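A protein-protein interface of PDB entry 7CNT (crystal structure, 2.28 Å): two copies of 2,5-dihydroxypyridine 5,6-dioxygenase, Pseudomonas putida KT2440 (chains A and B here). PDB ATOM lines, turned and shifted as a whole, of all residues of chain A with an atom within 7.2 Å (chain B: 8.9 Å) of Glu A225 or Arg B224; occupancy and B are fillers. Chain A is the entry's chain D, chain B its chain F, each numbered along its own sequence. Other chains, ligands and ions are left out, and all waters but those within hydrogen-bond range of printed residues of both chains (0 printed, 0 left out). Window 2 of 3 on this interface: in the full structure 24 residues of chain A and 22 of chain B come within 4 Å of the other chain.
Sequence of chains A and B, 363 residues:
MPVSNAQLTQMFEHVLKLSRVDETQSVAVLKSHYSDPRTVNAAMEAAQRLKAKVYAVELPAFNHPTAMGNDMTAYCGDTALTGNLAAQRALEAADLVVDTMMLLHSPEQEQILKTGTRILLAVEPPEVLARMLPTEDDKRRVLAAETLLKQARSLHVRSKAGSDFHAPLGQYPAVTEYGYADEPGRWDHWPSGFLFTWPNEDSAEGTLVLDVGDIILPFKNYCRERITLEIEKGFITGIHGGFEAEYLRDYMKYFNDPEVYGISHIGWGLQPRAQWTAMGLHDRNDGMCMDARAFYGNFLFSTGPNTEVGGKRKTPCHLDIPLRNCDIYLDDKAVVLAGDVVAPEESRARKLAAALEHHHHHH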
ATOM      1  N   LEU A 210     -39.576  -1.484 -12.675  1.00  0.00           N
ATOM      2  CA  LEU A 210     -38.148  -1.219 -12.841  1.00  0.00           C
ATOM      3  C   LEU A 210     -37.627  -2.160 -13.918  1.00  0.00           C
ATOM      4  O   LEU A 210     -37.490  -3.343 -13.689  1.00  0.00           O
ATOM      5  CB  LEU A 210     -37.398  -1.472 -11.545  1.00  0.00           C
ATOM      6  CG  LEU A 210     -37.577  -0.489 -10.375  1.00  0.00           C
ATOM      7  CD1 LEU A 210     -38.947  -0.470  -9.720  1.00  0.00           C
ATOM      8  CD2 LEU A 210     -36.541  -0.816  -9.310  1.00  0.00           C
ATOM      9  N   ASP A 211     -37.368  -1.629 -15.101  1.00  0.00           N
ATOM     10  CA  ASP A 211     -36.896  -2.410 -16.250  1.00  0.00           C
ATOM     11  C   ASP A 211     -35.488  -2.825 -15.942  1.00  0.00           C
ATOM     12  O   ASP A 211     -34.875  -2.358 -14.979  1.00  0.00           O
ATOM     13  CB  ASP A 211     -36.908  -1.544 -17.558  1.00  0.00           C
ATOM     14  CG  ASP A 211     -36.959  -2.389 -18.896  1.00  0.00           C
ATOM     15  OD1 ASP A 211     -36.945  -3.641 -18.843  1.00  0.00           O
ATOM     16  OD2 ASP A 211     -37.026  -1.783 -20.018  1.00  0.00           O
ATOM     17  N   VAL A 212     -34.975  -3.685 -16.794  1.00  0.00           N
ATOM     18  CA  VAL A 212     -33.548  -3.900 -16.881  1.00  0.00           C
ATOM     19  C   VAL A 212     -32.912  -2.539 -17.128  1.00  0.00           C
ATOM     20  O   VAL A 212     -33.291  -1.828 -18.036  1.00  0.00           O
ATOM     21  CB  VAL A 212     -33.170  -4.865 -18.015  1.00  0.00           C
ATOM     22  CG1 VAL A 212     -31.651  -4.974 -18.110  1.00  0.00           C
ATOM     23  CG2 VAL A 212     -33.799  -6.259 -17.806  1.00  0.00           C
ATOM     24  N   GLY A 213     -31.962  -2.164 -16.281  1.00  0.00           N
ATOM     25  CA  GLY A 213     -31.226  -0.935 -16.486  1.00  0.00           C
ATOM     26  C   GLY A 213     -31.722   0.190 -15.638  1.00  0.00           C
ATOM     27  O   GLY A 213     -31.139   1.272 -15.659  1.00  0.00           O
ATOM     28  N   ASP A 214     -32.821  -0.025 -14.922  1.00  0.00           N
ATOM     29  CA  ASP A 214     -33.307   1.008 -14.015  1.00  0.00           C
ATOM     30  C   ASP A 214     -32.552   0.837 -12.720  1.00  0.00           C
ATOM     31  O   ASP A 214     -31.851  -0.169 -12.527  1.00  0.00           O
ATOM     32  CB  ASP A 214     -34.816   0.957 -13.827  1.00  0.00           C
ATOM     33  CG  ASP A 214     -35.569   1.425 -15.047  1.00  0.00           C
ATOM     34  OD1 ASP A 214     -35.041   2.228 -15.852  1.00  0.00           O
ATOM     35  OD2 ASP A 214     -36.716   0.995 -15.222  1.00  0.00           O
ATOM     36  N   ASN A 221     -27.353  -0.020  -8.035  1.00  0.00           N
ATOM     37  CA  ASN A 221     -27.193  -1.009  -9.093  1.00  0.00           C
ATOM     38  C   ASN A 221     -28.116  -0.716 -10.265  1.00  0.00           C
ATOM     39  O   ASN A 221     -29.160  -0.087 -10.117  1.00  0.00           O
ATOM     40  CB  ASN A 221     -27.445  -2.430  -8.578  1.00  0.00           C
ATOM     41  CG  ASN A 221     -26.544  -2.798  -7.412  1.00  0.00           C
ATOM     42  OD1 ASN A 221     -25.392  -2.342  -7.302  1.00  0.00           O
ATOM     43  ND2 ASN A 221     -27.066  -3.638  -6.526  1.00  0.00           N
ATOM     44  N   TYR A 222     -27.661  -1.124 -11.443  1.00  0.00           N
ATOM     45  CA  TYR A 222     -28.493  -1.215 -12.597  1.00  0.00           C
ATOM     46  C   TYR A 222     -29.176  -2.572 -12.456  1.00  0.00           C
ATOM     47  O   TYR A 222     -28.498  -3.600 -12.347  1.00  0.00           O
ATOM     48  CB  TYR A 222     -27.657  -1.181 -13.867  1.00  0.00           C
ATOM     49  CG  TYR A 222     -26.922   0.111 -14.085  1.00  0.00           C
ATOM     50  CD1 TYR A 222     -27.556   1.180 -14.659  1.00  0.00           C
ATOM     51  CD2 TYR A 222     -25.598   0.274 -13.690  1.00  0.00           C
ATOM     52  CE1 TYR A 222     -26.908   2.372 -14.845  1.00  0.00           C
ATOM     53  CE2 TYR A 222     -24.934   1.473 -13.892  1.00  0.00           C
ATOM     54  CZ  TYR A 222     -25.589   2.522 -14.488  1.00  0.00           C
ATOM     55  OH  TYR A 222     -24.960   3.744 -14.711  1.00  0.00           O
ATOM     56  N   CYS A 223     -30.506  -2.578 -12.433  1.00  0.00           N
ATOM     57  CA  CYS A 223     -31.235  -3.853 -12.343  1.00  0.00           C
ATOM     58  C   CYS A 223     -30.938  -4.687 -13.566  1.00  0.00           C
ATOM     59  O   CYS A 223     -30.943  -4.166 -14.672  1.00  0.00           O
ATOM     60  CB  CYS A 223     -32.743  -3.640 -12.272  1.00  0.00           C
ATOM     61  SG  CYS A 223     -33.284  -2.734 -10.804  1.00  0.00           S
ATOM     62  N   ARG A 224     -30.669  -5.970 -13.338  1.00  0.00           N
ATOM     63  CA  ARG A 224     -30.443  -6.948 -14.398  1.00  0.00           C
ATOM     64  C   ARG A 224     -31.661  -7.807 -14.718  1.00  0.00           C
ATOM     65  O   ARG A 224     -31.714  -8.442 -15.780  1.00  0.00           O
ATOM     66  CB  ARG A 224     -29.239  -7.849 -14.031  1.00  0.00           C
ATOM     67  CG  ARG A 224     -27.926  -7.089 -13.822  1.00  0.00           C
ATOM     68  CD  ARG A 224     -27.632  -6.177 -15.026  1.00  0.00           C
ATOM     69  NE  ARG A 224     -27.619  -6.957 -16.275  1.00  0.00           N
ATOM     70  CZ  ARG A 224     -26.520  -7.294 -16.950  1.00  0.00           C
ATOM     71  NH1 ARG A 224     -25.322  -6.901 -16.530  1.00  0.00           N
ATOM     72  NH2 ARG A 224     -26.620  -8.029 -18.049  1.00  0.00           N
ATOM     73  N   GLU A 225     -32.593  -7.874 -13.768  1.00  0.00           N
ATOM     74  CA  GLU A 225     -33.939  -8.397 -14.001  1.00  0.00           C
ATOM     75  C   GLU A 225     -34.996  -7.336 -13.611  1.00  0.00           C
ATOM     76  O   GLU A 225     -34.711  -6.423 -12.832  1.00  0.00           O
ATOM     77  CB  GLU A 225     -34.178  -9.654 -13.184  1.00  0.00           C
ATOM     78  CG  GLU A 225     -33.130 -10.735 -13.349  1.00  0.00           C
ATOM     79  CD  GLU A 225     -32.976 -11.579 -12.093  1.00  0.00           C
ATOM     80  OE1 GLU A 225     -32.929 -11.006 -10.983  1.00  0.00           O
ATOM     81  OE2 GLU A 225     -32.892 -12.811 -12.207  1.00  0.00           O
ATOM     82  N   ARG A 226     -36.193  -7.469 -14.186  1.00  0.00           N
ATOM     83  CA  ARG A 226     -37.326  -6.605 -13.904  1.00  0.00           C
ATOM     84  C   ARG A 226     -37.797  -6.780 -12.462  1.00  0.00           C
ATOM     85  O   ARG A 226     -37.747  -7.865 -11.914  1.00  0.00           O
ATOM     86  CB  ARG A 226     -38.482  -6.945 -14.826  1.00  0.00           C
ATOM     87  CG  ARG A 226     -38.347  -6.378 -16.215  1.00  0.00           C
ATOM     88  CD  ARG A 226     -39.592  -6.601 -17.064  1.00  0.00           C
ATOM     89  NE  ARG A 226     -39.310  -6.199 -18.442  1.00  0.00           N
ATOM     90  CZ  ARG A 226     -40.194  -6.205 -19.441  1.00  0.00           C
ATOM     91  NH1 ARG A 226     -41.454  -6.598 -19.241  1.00  0.00           N
ATOM     92  NH2 ARG A 226     -39.813  -5.805 -20.653  1.00  0.00           N
ATOM     93  N   ILE A 227     -38.230  -5.692 -11.853  1.00  0.00           N
ATOM     94  CA  ILE A 227     -38.986  -5.766 -10.626  1.00  0.00           C
ATOM     95  C   ILE A 227     -40.308  -5.074 -10.894  1.00  0.00           C
ATOM     96  O   ILE A 227     -40.326  -3.920 -11.287  1.00  0.00           O
ATOM     97  CB  ILE A 227     -38.316  -5.037  -9.451  1.00  0.00           C
ATOM     98  CG1 ILE A 227     -36.934  -5.595  -9.187  1.00  0.00           C
ATOM     99  CG2 ILE A 227     -39.164  -5.145  -8.182  1.00  0.00           C
ATOM    100  CD1 ILE A 227     -36.169  -4.754  -8.188  1.00  0.00           C
ATOM    101  N   THR A 228     -41.409  -5.758 -10.617  1.00  0.00           N
ATOM    102  CA  THR A 228     -42.723  -5.135 -10.696  1.00  0.00           C
ATOM    103  C   THR A 228     -43.244  -4.740  -9.312  1.00  0.00           C
ATOM    104  O   THR A 228     -43.350  -5.561  -8.367  1.00  0.00           O
ATOM    105  CB  THR A 228     -43.669  -6.062 -11.444  1.00  0.00           C
ATOM    106  OG1 THR A 228     -43.126  -6.268 -12.760  1.00  0.00           O
ATOM    107  CG2 THR A 228     -45.057  -5.460 -11.564  1.00  0.00           C
ATOM    108  N   HIS A 240     -42.300  -8.027  -7.062  1.00  0.00           N
ATOM    109  CA  HIS A 240     -42.157  -9.284  -7.804  1.00  0.00           C
ATOM    110  C   HIS A 240     -41.017  -9.199  -8.804  1.00  0.00           C
ATOM    111  O   HIS A 240     -40.680  -8.118  -9.278  1.00  0.00           O
ATOM    112  CB  HIS A 240     -43.449  -9.595  -8.585  1.00  0.00           C
ATOM    113  CG  HIS A 240     -44.694  -9.539  -7.753  1.00  0.00           C
ATOM    114  ND1 HIS A 240     -44.935 -10.417  -6.715  1.00  0.00           N
ATOM    115  CD2 HIS A 240     -45.769  -8.713  -7.806  1.00  0.00           C
ATOM    116  CE1 HIS A 240     -46.102 -10.136  -6.163  1.00  0.00           C
ATOM    117  NE2 HIS A 240     -46.627  -9.106  -6.805  1.00  0.00           N
ATOM    118  N   GLY A 241     -40.464 -10.350  -9.164  1.00  0.00           N
ATOM    119  CA  GLY A 241     -39.400 -10.431 -10.169  1.00  0.00           C
ATOM    120  C   GLY A 241     -38.366 -11.426  -9.721  1.00  0.00           C
ATOM    121  O   GLY A 241     -38.709 -12.403  -9.084  1.00  0.00           O
ATOM    122  N   GLY A 242     -37.096 -11.185 -10.032  1.00  0.00           N
ATOM    123  CA  GLY A 242     -36.041 -12.143  -9.665  1.00  0.00           C
ATOM    124  C   GLY A 242     -35.238 -11.791  -8.412  1.00  0.00           C
ATOM    125  O   GLY A 242     -35.776 -11.456  -7.370  1.00  0.00           O
ATOM    126  N   PHE A 243     -33.923 -11.872  -8.528  1.00  0.00           N
ATOM    127  CA  PHE A 243     -33.050 -11.727  -7.385  1.00  0.00           C
ATOM    128  C   PHE A 243     -33.107 -10.330  -6.806  1.00  0.00           C
ATOM    129  O   PHE A 243     -33.151 -10.175  -5.595  1.00  0.00           O
ATOM    130  CB  PHE A 243     -31.601 -12.121  -7.718  1.00  0.00           C
ATOM    131  CG  PHE A 243     -30.622 -11.599  -6.726  1.00  0.00           C
ATOM    132  CD1 PHE A 243     -30.550 -12.164  -5.475  1.00  0.00           C
ATOM    133  CD2 PHE A 243     -29.859 -10.476  -7.005  1.00  0.00           C
ATOM    134  CE1 PHE A 243     -29.699 -11.645  -4.523  1.00  0.00           C
ATOM    135  CE2 PHE A 243     -29.005  -9.947  -6.064  1.00  0.00           C
ATOM    136  CZ  PHE A 243     -28.928 -10.535  -4.817  1.00  0.00           C
ATOM    137  N   GLU A 244     -33.138  -9.320  -7.655  1.00  0.00           N
ATOM    138  CA  GLU A 244     -33.316  -7.959  -7.189  1.00  0.00           C
ATOM    139  C   GLU A 244     -34.594  -7.782  -6.332  1.00  0.00           C
ATOM    140  O   GLU A 244     -34.583  -7.098  -5.300  1.00  0.00           O
ATOM    141  CB  GLU A 244     -33.357  -6.983  -8.359  1.00  0.00           C
ATOM    142  CG  GLU A 244     -31.992  -6.578  -8.916  1.00  0.00           C
ATOM    143  CD  GLU A 244     -31.547  -7.351 -10.155  1.00  0.00           C
ATOM    144  OE1 GLU A 244     -30.582  -6.911 -10.777  1.00  0.00           O
ATOM    145  OE2 GLU A 244     -32.108  -8.405 -10.489  1.00  0.00           O
ATOM    146  N   ALA A 245     -35.673  -8.394  -6.792  1.00  0.00           N
ATOM    147  CA  ALA A 245     -36.964  -8.359  -6.129  1.00  0.00           C
ATOM    148  C   ALA A 245     -36.825  -8.864  -4.713  1.00  0.00           C
ATOM    149  O   ALA A 245     -37.326  -8.237  -3.804  1.00  0.00           O
ATOM    150  CB  ALA A 245     -37.976  -9.219  -6.891  1.00  0.00           C
ATOM    151  N   LEU B 210     -24.164 -23.246  -4.487  1.00  0.00           N
ATOM    152  CA  LEU B 210     -24.307 -21.815  -4.229  1.00  0.00           C
ATOM    153  C   LEU B 210     -25.443 -21.404  -5.099  1.00  0.00           C
ATOM    154  O   LEU B 210     -25.330 -21.430  -6.317  1.00  0.00           O
ATOM    155  CB  LEU B 210     -23.074 -21.003  -4.607  1.00  0.00           C
ATOM    156  CG  LEU B 210     -21.922 -21.055  -3.636  1.00  0.00           C
ATOM    157  CD1 LEU B 210     -21.405 -22.478  -3.478  1.00  0.00           C
ATOM    158  CD2 LEU B 210     -20.840 -20.146  -4.169  1.00  0.00           C
ATOM    159  N   ASP B 211     -26.544 -21.066  -4.467  1.00  0.00           N
ATOM    160  CA  ASP B 211     -27.728 -20.671  -5.158  1.00  0.00           C
ATOM    161  C   ASP B 211     -27.567 -19.230  -5.546  1.00  0.00           C
ATOM    162  O   ASP B 211     -26.610 -18.553  -5.132  1.00  0.00           O
ATOM    163  CB  ASP B 211     -28.935 -20.800  -4.214  1.00  0.00           C
ATOM    164  CG  ASP B 211     -30.278 -20.780  -4.953  1.00  0.00           C
ATOM    165  OD1 ASP B 211     -30.282 -20.879  -6.220  1.00  0.00           O
ATOM    166  OD2 ASP B 211     -31.325 -20.653  -4.251  1.00  0.00           O
ATOM    167  N   VAL B 212     -28.541 -18.762  -6.309  1.00  0.00           N
ATOM    168  CA  VAL B 212     -28.722 -17.351  -6.580  1.00  0.00           C
ATOM    169  C   VAL B 212     -28.789 -16.579  -5.265  1.00  0.00           C
ATOM    170  O   VAL B 212     -29.573 -16.933  -4.374  1.00  0.00           O
ATOM    171  CB  VAL B 212     -30.011 -17.130  -7.435  1.00  0.00           C
ATOM    172  CG1 VAL B 212     -30.356 -15.648  -7.588  1.00  0.00           C
ATOM    173  CG2 VAL B 212     -29.843 -17.754  -8.815  1.00  0.00           C
ATOM    174  N   GLY B 213     -27.961 -15.536  -5.153  1.00  0.00           N
ATOM    175  CA  GLY B 213     -27.929 -14.690  -3.977  1.00  0.00           C
ATOM    176  C   GLY B 213     -26.963 -15.139  -2.898  1.00  0.00           C
ATOM    177  O   GLY B 213     -26.665 -14.371  -1.983  1.00  0.00           O
ATOM    178  N   ASP B 214     -26.455 -16.366  -2.975  1.00  0.00           N
ATOM    179  CA  ASP B 214     -25.394 -16.778  -2.060  1.00  0.00           C
ATOM    180  C   ASP B 214     -24.071 -16.094  -2.418  1.00  0.00           C
ATOM    181  O   ASP B 214     -23.935 -15.517  -3.502  1.00  0.00           O
ATOM    182  CB  ASP B 214     -25.292 -18.297  -1.955  1.00  0.00           C
ATOM    183  CG  ASP B 214     -26.528 -18.917  -1.280  1.00  0.00           C
ATOM    184  OD1 ASP B 214     -27.072 -18.313  -0.296  1.00  0.00           O
ATOM    185  OD2 ASP B 214     -26.965 -20.000  -1.751  1.00  0.00           O
ATOM    186  N   ILE B 215     -23.133 -16.083  -1.467  1.00  0.00           N
ATOM    187  CA  ILE B 215     -21.964 -15.185  -1.543  1.00  0.00           C
ATOM    188  C   ILE B 215     -20.649 -15.914  -1.456  1.00  0.00           C
ATOM    189  O   ILE B 215     -20.491 -16.825  -0.610  1.00  0.00           O
ATOM    190  CB  ILE B 215     -21.935 -14.200  -0.349  1.00  0.00           C
ATOM    191  CG1 ILE B 215     -23.195 -13.358  -0.311  1.00  0.00           C
ATOM    192  CG2 ILE B 215     -20.710 -13.310  -0.422  1.00  0.00           C
ATOM    193  CD1 ILE B 215     -23.282 -12.481   0.910  1.00  0.00           C
ATOM    194  N   ASN B 221     -19.495 -10.880  -4.118  1.00  0.00           N
ATOM    195  CA  ASN B 221     -20.657 -10.847  -5.006  1.00  0.00           C
ATOM    196  C   ASN B 221     -21.781 -11.753  -4.616  1.00  0.00           C
ATOM    197  O   ASN B 221     -21.544 -12.901  -4.237  1.00  0.00           O
ATOM    198  CB  ASN B 221     -20.261 -11.391  -6.364  1.00  0.00           C
ATOM    199  CG  ASN B 221     -19.195 -10.599  -6.965  1.00  0.00           C
ATOM    200  OD1 ASN B 221     -19.238  -9.376  -6.903  1.00  0.00           O
ATOM    201  ND2 ASN B 221     -18.216 -11.261  -7.520  1.00  0.00           N
ATOM    202  N   TYR B 222     -22.998 -11.275  -4.873  1.00  0.00           N
ATOM    203  CA  TYR B 222     -24.176 -12.117  -4.804  1.00  0.00           C
ATOM    204  C   TYR B 222     -24.165 -12.957  -6.062  1.00  0.00           C
ATOM    205  O   TYR B 222     -24.269 -12.399  -7.145  1.00  0.00           O
ATOM    206  CB  TYR B 222     -25.453 -11.258  -4.735  1.00  0.00           C
ATOM    207  CG  TYR B 222     -25.549 -10.471  -3.449  1.00  0.00           C
ATOM    208  CD1 TYR B 222     -25.909 -11.099  -2.257  1.00  0.00           C
ATOM    209  CD2 TYR B 222     -25.237  -9.136  -3.404  1.00  0.00           C
ATOM    210  CE1 TYR B 222     -26.005 -10.384  -1.077  1.00  0.00           C
ATOM    211  CE2 TYR B 222     -25.307  -8.415  -2.229  1.00  0.00           C
ATOM    212  CZ  TYR B 222     -25.708  -9.046  -1.070  1.00  0.00           C
ATOM    213  OH  TYR B 222     -25.741  -8.350   0.114  1.00  0.00           O
ATOM    214  N   CYS B 223     -24.009 -14.278  -5.940  1.00  0.00           N
ATOM    215  CA  CYS B 223     -24.149 -15.133  -7.122  1.00  0.00           C
ATOM    216  C   CYS B 223     -25.454 -14.876  -7.882  1.00  0.00           C
ATOM    217  O   CYS B 223     -26.540 -14.727  -7.287  1.00  0.00           O
ATOM    218  CB  CYS B 223     -24.060 -16.597  -6.749  1.00  0.00           C
ATOM    219  SG  CYS B 223     -22.500 -16.983  -5.979  1.00  0.00           S
ATOM    220  N   ARG B 224     -25.358 -14.798  -9.206  1.00  0.00           N
ATOM    221  CA  ARG B 224     -26.562 -14.604 -10.037  1.00  0.00           C
ATOM    222  C   ARG B 224     -26.927 -15.901 -10.790  1.00  0.00           C
ATOM    223  O   ARG B 224     -28.015 -16.027 -11.401  1.00  0.00           O
ATOM    224  CB  ARG B 224     -26.314 -13.447 -11.003  1.00  0.00           C
ATOM    225  CG  ARG B 224     -25.959 -12.113 -10.316  1.00  0.00           C
ATOM    226  CD  ARG B 224     -27.085 -11.590  -9.411  1.00  0.00           C
ATOM    227  NE  ARG B 224     -28.355 -11.569 -10.126  1.00  0.00           N
ATOM    228  CZ  ARG B 224     -28.961 -10.480 -10.610  1.00  0.00           C
ATOM    229  NH1 ARG B 224     -28.446  -9.249 -10.424  1.00  0.00           N
ATOM    230  NH2 ARG B 224     -30.118 -10.621 -11.274  1.00  0.00           N
ATOM    231  N   GLU B 225     -25.986 -16.845 -10.790  1.00  0.00           N
ATOM    232  CA  GLU B 225     -26.172 -18.166 -11.404  1.00  0.00           C
ATOM    233  C   GLU B 225     -25.580 -19.168 -10.451  1.00  0.00           C
ATOM    234  O   GLU B 225     -24.537 -18.911  -9.809  1.00  0.00           O
ATOM    235  CB  GLU B 225     -25.416 -18.326 -12.741  1.00  0.00           C
ATOM    236  CG  GLU B 225     -25.553 -17.219 -13.785  1.00  0.00           C
ATOM    237  CD  GLU B 225     -24.488 -17.312 -14.901  1.00  0.00           C
ATOM    238  OE1 GLU B 225     -23.265 -17.309 -14.604  1.00  0.00           O
ATOM    239  OE2 GLU B 225     -24.868 -17.376 -16.092  1.00  0.00           O
ATOM    240  N   ARG B 226     -26.207 -20.324 -10.396  1.00  0.00           N
ATOM    241  CA  ARG B 226     -25.798 -21.390  -9.510  1.00  0.00           C
ATOM    242  C   ARG B 226     -24.399 -21.854  -9.758  1.00  0.00           C
ATOM    243  O   ARG B 226     -23.969 -21.895 -10.874  1.00  0.00           O
ATOM    244  CB  ARG B 226     -26.738 -22.587  -9.640  1.00  0.00           C
ATOM    245  CG  ARG B 226     -28.042 -22.327  -8.918  1.00  0.00           C
ATOM    246  CD  ARG B 226     -29.016 -23.487  -9.008  1.00  0.00           C
ATOM    247  NE  ARG B 226     -30.309 -23.093  -8.443  1.00  0.00           N
ATOM    248  CZ  ARG B 226     -31.264 -23.931  -8.059  1.00  0.00           C
ATOM    249  NH1 ARG B 226     -31.096 -25.245  -8.159  1.00  0.00           N
ATOM    250  NH2 ARG B 226     -32.396 -23.441  -7.562  1.00  0.00           N
ATOM    251  N   ILE B 227     -23.703 -22.187  -8.681  1.00  0.00           N
ATOM    252  CA  ILE B 227     -22.465 -22.926  -8.719  1.00  0.00           C
ATOM    253  C   ILE B 227     -22.662 -24.192  -7.905  1.00  0.00           C
ATOM    254  O   ILE B 227     -23.164 -24.168  -6.775  1.00  0.00           O
ATOM    255  CB  ILE B 227     -21.264 -22.116  -8.161  1.00  0.00           C
ATOM    256  CG1 ILE B 227     -21.116 -20.771  -8.884  1.00  0.00           C
ATOM    257  CG2 ILE B 227     -19.972 -22.934  -8.328  1.00  0.00           C
ATOM    258  CD1 ILE B 227     -19.880 -19.989  -8.507  1.00  0.00           C
ATOM    259  N   GLY B 242     -22.273 -21.639 -14.647  1.00  0.00           N
ATOM    260  CA  GLY B 242     -21.964 -20.610 -15.647  1.00  0.00           C
ATOM    261  C   GLY B 242     -20.677 -19.823 -15.377  1.00  0.00           C
ATOM    262  O   GLY B 242     -19.622 -20.405 -15.140  1.00  0.00           O
ATOM    263  N   PHE B 243     -20.778 -18.499 -15.401  1.00  0.00           N
ATOM    264  CA  PHE B 243     -19.624 -17.608 -15.319  1.00  0.00           C
ATOM    265  C   PHE B 243     -19.017 -17.496 -13.913  1.00  0.00           C
ATOM    266  O   PHE B 243     -17.795 -17.360 -13.747  1.00  0.00           O
ATOM    267  CB  PHE B 243     -20.045 -16.208 -15.756  1.00  0.00           C
ATOM    268  CG  PHE B 243     -19.079 -15.160 -15.353  1.00  0.00           C
ATOM    269  CD1 PHE B 243     -17.874 -15.046 -16.022  1.00  0.00           C
ATOM    270  CD2 PHE B 243     -19.334 -14.314 -14.293  1.00  0.00           C
ATOM    271  CE1 PHE B 243     -16.964 -14.077 -15.660  1.00  0.00           C
ATOM    272  CE2 PHE B 243     -18.419 -13.334 -13.912  1.00  0.00           C
ATOM    273  CZ  PHE B 243     -17.234 -13.214 -14.605  1.00  0.00           C
ATOM    274  N   GLU B 244     -19.850 -17.522 -12.879  1.00  0.00           N
ATOM    275  CA  GLU B 244     -19.268 -17.470 -11.526  1.00  0.00           C
ATOM    276  C   GLU B 244     -18.428 -18.706 -11.293  1.00  0.00           C
ATOM    277  O   GLU B 244     -17.389 -18.666 -10.677  1.00  0.00           O
ATOM    278  CB  GLU B 244     -20.324 -17.319 -10.429  1.00  0.00           C
ATOM    279  CG  GLU B 244     -20.941 -15.932 -10.294  1.00  0.00           C
ATOM    280  CD  GLU B 244     -22.281 -15.752 -10.999  1.00  0.00           C
ATOM    281  OE1 GLU B 244     -22.939 -14.719 -10.713  1.00  0.00           O
ATOM    282  OE2 GLU B 244     -22.669 -16.609 -11.837  1.00  0.00           O
ATOM    283  N   ALA B 245     -18.861 -19.821 -11.823  1.00  0.00           N
ATOM    284  CA  ALA B 245     -18.101 -21.032 -11.662  1.00  0.00           C
ATOM    285  C   ALA B 245     -16.765 -20.954 -12.419  1.00  0.00           C
ATOM    286  O   ALA B 245     -15.733 -21.393 -11.917  1.00  0.00           O
ATOM    287  CB  ALA B 245     -18.954 -22.236 -12.118  1.00  0.00           C
ATOM    288  N   TRP B 276     -27.672 -10.121   5.542  1.00  0.00           N
ATOM    289  CA  TRP B 276     -27.261 -10.697   4.318  1.00  0.00           C
ATOM    290  C   TRP B 276     -27.255  -9.619   3.244  1.00  0.00           C
ATOM    291  O   TRP B 276     -26.571  -9.784   2.282  1.00  0.00           O
ATOM    292  CB  TRP B 276     -28.239 -11.843   3.940  1.00  0.00           C
ATOM    293  CG  TRP B 276     -28.216 -12.237   2.509  1.00  0.00           C
ATOM    294  CD1 TRP B 276     -27.273 -13.011   1.882  1.00  0.00           C
ATOM    295  CD2 TRP B 276     -29.167 -11.864   1.498  1.00  0.00           C
ATOM    296  NE1 TRP B 276     -27.592 -13.157   0.540  1.00  0.00           N
ATOM    297  CE2 TRP B 276     -28.744 -12.460   0.282  1.00  0.00           C
ATOM    298  CE3 TRP B 276     -30.345 -11.113   1.508  1.00  0.00           C
ATOM    299  CZ2 TRP B 276     -29.442 -12.295  -0.917  1.00  0.00           C
ATOM    300  CZ3 TRP B 276     -31.048 -10.946   0.302  1.00  0.00           C
ATOM    301  CH2 TRP B 276     -30.597 -11.547  -0.888  1.00  0.00           C
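NH2 of Arg B224 lies within salt-bridge range of OE1 of Glu A225 (2.9 Å).
NH2 of Arg B224 is in salt-bridge range of OE2 of Glu A244 (3.1 Å).
N of Arg A224 is in hydrogen-bond range of OE1 of Glu A244 (2.7 Å).
The side-chain carboxylate (OE1) of Glu A225 sits at hydrogen-bond distance from the backbone NH (N) of Phe A243 (2.8 Å).
The backbone NH (N) of Glu A225 sits at hydrogen-bond distance from the side-chain carboxylate (OE2) of Glu A244, 3.4 Å away.
The backbone carbonyl oxygen (O) of Gly B213 sits at hydrogen-bond distance from the indole nitrogen (NE1) of Trp B276, at 2.9 Å.
The backbone carbonyl oxygen (O) of Trp B276 sits at hydrogen-bond distance from the side-chain hydroxyl (OH) of Tyr B222 (2.7 Å).
OE1 of Glu B244 lies within hydrogen-bond range of N of Arg B224 (2.9 Å).
Among the printed residues, merely in contact across the chains: Arg A224 with Arg B224 (3.9 Å), Phe A243 with Val B212 (3.7 Å), Phe A243 with Gly B213 (3.6 Å), Phe A243 with Tyr B222 (3.6 Å), Phe A243 with Arg B224 (3.6 Å) and Phe A243 with Trp B276 (3.7 Å).
Printed residues of chain B within 4 Å of Arg A224: Arg B224 (3.9 Å).
Glu A225 touches one residue of chain B.
Of the printed residues of chain B, Phe A243 touches Val B212, Gly B213, Tyr B222, Arg B224 and Trp B276.
Of the printed residues of chain B, Glu A244 touches Arg B224 (3.1 Å).
Of the printed residues of chain A, Gly B213 touches Phe A243 (3.6 Å).
Of chain A, only Arg A224, Glu A225, Phe A243 and Glu A244 come within 4 Å of Arg B224.
Phe B243 touches none of the printed residues of chain A.
The nearest printed residue of chain A that does not touch Trp B276 is Glu A244 (7.4 Å).
Of the 19 printed residues of chain A, 4 touch a printed residue of chain B.
Hydrophobic or aromatic side chains of chain A that line the printed part of chain B: Phe A243.
Along chain A the printed residues that touch a printed residue of chain B span positions 224 to 244.
Printed residues of chain B that touch a printed residue of chain A: Val B212, Gly B213, Tyr B222, Arg B224 and Trp B276.
Along chain B the printed residues that touch a printed residue of chain A span positions 212 to 276.
Among the printed residues, 8 pairs touch across the chains.
Arg A224 touches its own counterpart, Arg B224.
Phe A243 touches Val B212, but with the chains exchanged Val A212 does not touch Phe B243 (15.9 Å).
Phe A243 touches Arg B224, but with the chains exchanged Arg A224 does not touch Phe B243 (9.8 Å).
Glu A244 touches Arg B224, but with the chains exchanged Arg A224 does not touch Glu B244 (9.6 Å).
Positions printed for both chains: 210, 211, 212, 213, 214, 221, 222, 223, 224, 225, 226, 227, 242, 243, 244 and 245.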
